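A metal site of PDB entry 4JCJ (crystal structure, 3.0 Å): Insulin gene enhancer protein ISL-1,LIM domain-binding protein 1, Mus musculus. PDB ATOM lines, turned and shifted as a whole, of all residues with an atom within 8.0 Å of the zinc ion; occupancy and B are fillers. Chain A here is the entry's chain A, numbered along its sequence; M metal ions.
The side-chain sulfur (SG) of Cys 102 lies close to the guanidinium group (NE) of Arg 104 (3.1 Å).
N of Ala 101 sits close to SG of Cys 99 (3.5 Å).
N of Cys 99 is in hydrogen-bond range of O of Arg 104 (2.8 Å).
SG of Cys 121 sits close to NH2 of Arg 104 (3.7 Å).
N of Ala 123 lies close to SG of Cys 121 (3.7 Å).
The zinc ion is bound by OD2 of Asp 124 (2.0 Å), SG of Cys 102 (2.3 Å), SG of Cys 99 (2.3 Å) and SG of Cys 121 (2.3 Å).
The zinc ion has four donor atoms within binding distance.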
ATOM      1  N   ARG A  98     -21.185 -33.413   0.109  1.00  0.00           N
ATOM      2  CA  ARG A  98     -20.677 -33.474   1.480  1.00  0.00           C
ATOM      3  C   ARG A  98     -19.732 -32.307   1.703  1.00  0.00           C
ATOM      4  O   ARG A  98     -19.069 -31.838   0.769  1.00  0.00           O
ATOM      5  CB  ARG A  98     -19.917 -34.791   1.737  1.00  0.00           C
ATOM      6  CG  ARG A  98     -20.570 -36.069   1.201  1.00  0.00           C
ATOM      7  CD  ARG A  98     -21.950 -36.309   1.759  1.00  0.00           C
ATOM      8  NE  ARG A  98     -21.931 -37.109   2.980  1.00  0.00           N
ATOM      9  CZ  ARG A  98     -22.053 -38.434   3.031  1.00  0.00           C
ATOM     10  NH1 ARG A  98     -22.192 -39.171   1.923  1.00  0.00           N
ATOM     11  NH2 ARG A  98     -22.026 -39.052   4.195  1.00  0.00           N
ATOM     12  N   CYS A  99     -19.652 -31.839   2.935  1.00  0.00           N
ATOM     13  CA  CYS A  99     -18.621 -30.888   3.276  1.00  0.00           C
ATOM     14  C   CYS A  99     -17.283 -31.645   3.354  1.00  0.00           C
ATOM     15  O   CYS A  99     -17.175 -32.640   4.074  1.00  0.00           O
ATOM     16  CB  CYS A  99     -18.946 -30.172   4.585  1.00  0.00           C
ATOM     17  SG  CYS A  99     -17.538 -29.347   5.251  1.00  0.00           S
ATOM     18  N   VAL A 100     -16.289 -31.162   2.615  1.00  0.00           N
ATOM     19  CA  VAL A 100     -15.023 -31.881   2.494  1.00  0.00           C
ATOM     20  C   VAL A 100     -14.257 -31.930   3.819  1.00  0.00           C
ATOM     21  O   VAL A 100     -13.469 -32.844   4.041  1.00  0.00           O
ATOM     22  CB  VAL A 100     -14.094 -31.287   1.385  1.00  0.00           C
ATOM     23  CG1 VAL A 100     -12.940 -32.243   1.089  1.00  0.00           C
ATOM     24  CG2 VAL A 100     -14.876 -31.009   0.092  1.00  0.00           C
ATOM     25  N   ALA A 101     -14.497 -30.949   4.674  1.00  0.00           N
ATOM     26  CA  ALA A 101     -13.844 -30.857   5.982  1.00  0.00           C
ATOM     27  C   ALA A 101     -14.467 -31.776   7.030  1.00  0.00           C
ATOM     28  O   ALA A 101     -13.797 -32.663   7.534  1.00  0.00           O
ATOM     29  CB  ALA A 101     -13.868 -29.442   6.493  1.00  0.00           C
ATOM     30  N   CYS A 102     -15.743 -31.553   7.361  1.00  0.00           N
ATOM     31  CA  CYS A 102     -16.420 -32.386   8.358  1.00  0.00           C
ATOM     32  C   CYS A 102     -17.019 -33.628   7.739  1.00  0.00           C
ATOM     33  O   CYS A 102     -17.527 -34.503   8.456  1.00  0.00           O
ATOM     34  CB  CYS A 102     -17.517 -31.622   9.088  1.00  0.00           C
ATOM     35  SG  CYS A 102     -18.680 -30.916   7.970  1.00  0.00           S
ATOM     36  N   SER A 103     -16.963 -33.703   6.404  1.00  0.00           N
ATOM     37  CA  SER A 103     -17.257 -34.950   5.698  1.00  0.00           C
ATOM     38  C   SER A 103     -18.600 -35.446   6.137  1.00  0.00           C
ATOM     39  O   SER A 103     -18.743 -36.549   6.668  1.00  0.00           O
ATOM     40  CB  SER A 103     -16.183 -35.992   5.977  1.00  0.00           C
ATOM     41  OG  SER A 103     -16.366 -37.107   5.126  1.00  0.00           O
ATOM     42  N   ARG A 104     -19.581 -34.569   5.947  1.00  0.00           N
ATOM     43  CA  ARG A 104     -20.954 -34.875   6.298  1.00  0.00           C
ATOM     44  C   ARG A 104     -21.864 -34.131   5.326  1.00  0.00           C
ATOM     45  O   ARG A 104     -21.421 -33.182   4.666  1.00  0.00           O
ATOM     46  CB  ARG A 104     -21.231 -34.489   7.749  1.00  0.00           C
ATOM     47  CG  ARG A 104     -21.520 -33.041   7.980  1.00  0.00           C
ATOM     48  CD  ARG A 104     -21.502 -32.671   9.452  1.00  0.00           C
ATOM     49  NE  ARG A 104     -21.351 -31.216   9.591  1.00  0.00           N
ATOM     50  CZ  ARG A 104     -21.923 -30.454  10.519  1.00  0.00           C
ATOM     51  NH1 ARG A 104     -22.739 -30.975  11.439  1.00  0.00           N
ATOM     52  NH2 ARG A 104     -21.688 -29.140  10.520  1.00  0.00           N
ATOM     53  N   GLN A 105     -23.112 -34.561   5.252  1.00  0.00           N
ATOM     54  CA  GLN A 105     -24.011 -34.145   4.184  1.00  0.00           C
ATOM     55  C   GLN A 105     -24.507 -32.712   4.322  1.00  0.00           C
ATOM     56  O   GLN A 105     -24.546 -32.170   5.424  1.00  0.00           O
ATOM     57  CB  GLN A 105     -25.200 -35.112   4.114  1.00  0.00           C
ATOM     58  CG  GLN A 105     -26.096 -34.915   2.902  1.00  0.00           C
ATOM     59  CD  GLN A 105     -26.256 -36.179   2.084  1.00  0.00           C
ATOM     60  OE1 GLN A 105     -26.552 -37.254   2.609  1.00  0.00           O
ATOM     61  NE2 GLN A 105     -26.051 -36.042   0.772  1.00  0.00           N
ATOM     62  N   LEU A 106     -24.843 -32.100   3.201  1.00  0.00           N
ATOM     63  CA  LEU A 106     -25.458 -30.784   3.193  1.00  0.00           C
ATOM     64  C   LEU A 106     -26.913 -30.853   2.679  1.00  0.00           C
ATOM     65  O   LEU A 106     -27.212 -31.514   1.680  1.00  0.00           O
ATOM     66  CB  LEU A 106     -24.649 -29.823   2.340  1.00  0.00           C
ATOM     67  CG  LEU A 106     -23.219 -29.615   2.793  1.00  0.00           C
ATOM     68  CD1 LEU A 106     -22.591 -28.617   1.873  1.00  0.00           C
ATOM     69  CD2 LEU A 106     -23.131 -29.149   4.252  1.00  0.00           C
ATOM     70  N   LEU A 119     -16.541 -28.033  -1.123  1.00  0.00           N
ATOM     71  CA  LEU A 119     -17.689 -27.576  -0.369  1.00  0.00           C
ATOM     72  C   LEU A 119     -17.350 -27.531   1.119  1.00  0.00           C
ATOM     73  O   LEU A 119     -16.664 -28.418   1.635  1.00  0.00           O
ATOM     74  CB  LEU A 119     -18.883 -28.501  -0.609  1.00  0.00           C
ATOM     75  CG  LEU A 119     -19.425 -28.532  -2.041  1.00  0.00           C
ATOM     76  CD1 LEU A 119     -20.303 -29.743  -2.278  1.00  0.00           C
ATOM     77  CD2 LEU A 119     -20.201 -27.275  -2.369  1.00  0.00           C
ATOM     78  N   PHE A 120     -17.827 -26.497   1.784  1.00  0.00           N
ATOM     79  CA  PHE A 120     -17.630 -26.343   3.216  1.00  0.00           C
ATOM     80  C   PHE A 120     -18.916 -25.894   3.869  1.00  0.00           C
ATOM     81  O   PHE A 120     -19.615 -25.059   3.311  1.00  0.00           O
ATOM     82  CB  PHE A 120     -16.538 -25.326   3.508  1.00  0.00           C
ATOM     83  CG  PHE A 120     -15.190 -25.742   3.012  1.00  0.00           C
ATOM     84  CD1 PHE A 120     -14.820 -25.521   1.714  1.00  0.00           C
ATOM     85  CD2 PHE A 120     -14.293 -26.366   3.880  1.00  0.00           C
ATOM     86  CE1 PHE A 120     -13.578 -25.896   1.264  1.00  0.00           C
ATOM     87  CE2 PHE A 120     -13.042 -26.760   3.436  1.00  0.00           C
ATOM     88  CZ  PHE A 120     -12.680 -26.530   2.131  1.00  0.00           C
ATOM     89  N   CYS A 121     -19.208 -26.438   5.037  1.00  0.00           N
ATOM     90  CA  CYS A 121     -20.359 -26.000   5.813  1.00  0.00           C
ATOM     91  C   CYS A 121     -20.029 -24.680   6.516  1.00  0.00           C
ATOM     92  O   CYS A 121     -18.846 -24.358   6.723  1.00  0.00           O
ATOM     93  CB  CYS A 121     -20.731 -27.079   6.806  1.00  0.00           C
ATOM     94  SG  CYS A 121     -19.542 -27.275   8.118  1.00  0.00           S
ATOM     95  N   ARG A 122     -21.052 -23.916   6.905  1.00  0.00           N
ATOM     96  CA  ARG A 122     -20.834 -22.583   7.491  1.00  0.00           C
ATOM     97  C   ARG A 122     -20.071 -22.612   8.802  1.00  0.00           C
ATOM     98  O   ARG A 122     -19.776 -21.554   9.364  1.00  0.00           O
ATOM     99  CB  ARG A 122     -22.157 -21.860   7.695  1.00  0.00           C
ATOM    100  N   ALA A 123     -19.754 -23.799   9.316  1.00  0.00           N
ATOM    101  CA  ALA A 123     -18.895 -23.939  10.489  1.00  0.00           C
ATOM    102  C   ALA A 123     -17.433 -24.086  10.084  1.00  0.00           C
ATOM    103  O   ALA A 123     -16.562 -23.423  10.658  1.00  0.00           O
ATOM    104  CB  ALA A 123     -19.331 -25.131  11.318  1.00  0.00           C
ATOM    105  N   ASP A 124     -17.155 -24.952   9.127  1.00  0.00           N
ATOM    106  CA  ASP A 124     -15.775 -25.165   8.686  1.00  0.00           C
ATOM    107  C   ASP A 124     -15.257 -24.016   7.792  1.00  0.00           C
ATOM    108  O   ASP A 124     -14.046 -23.816   7.662  1.00  0.00           O
ATOM    109  CB  ASP A 124     -15.630 -26.537   7.993  1.00  0.00           C
ATOM    110  CG  ASP A 124     -15.928 -27.719   8.922  1.00  0.00           C
ATOM    111  OD1 ASP A 124     -16.003 -27.544  10.146  1.00  0.00           O
ATOM    112  OD2 ASP A 124     -16.070 -28.847   8.416  1.00  0.00           O
ATOM    113  N   HIS A 125     -16.163 -23.266   7.161  1.00  0.00           N
ATOM    114  CA  HIS A 125     -15.799 -22.061   6.418  1.00  0.00           C
ATOM    115  C   HIS A 125     -15.167 -21.022   7.345  1.00  0.00           C
ATOM    116  O   HIS A 125     -14.243 -20.319   6.956  1.00  0.00           O
ATOM    117  CB  HIS A 125     -17.028 -21.437   5.732  1.00  0.00           C
HETATM  118 ZN    ZN M   1     -17.867 -28.796   7.489  1.00  0.00          ZN
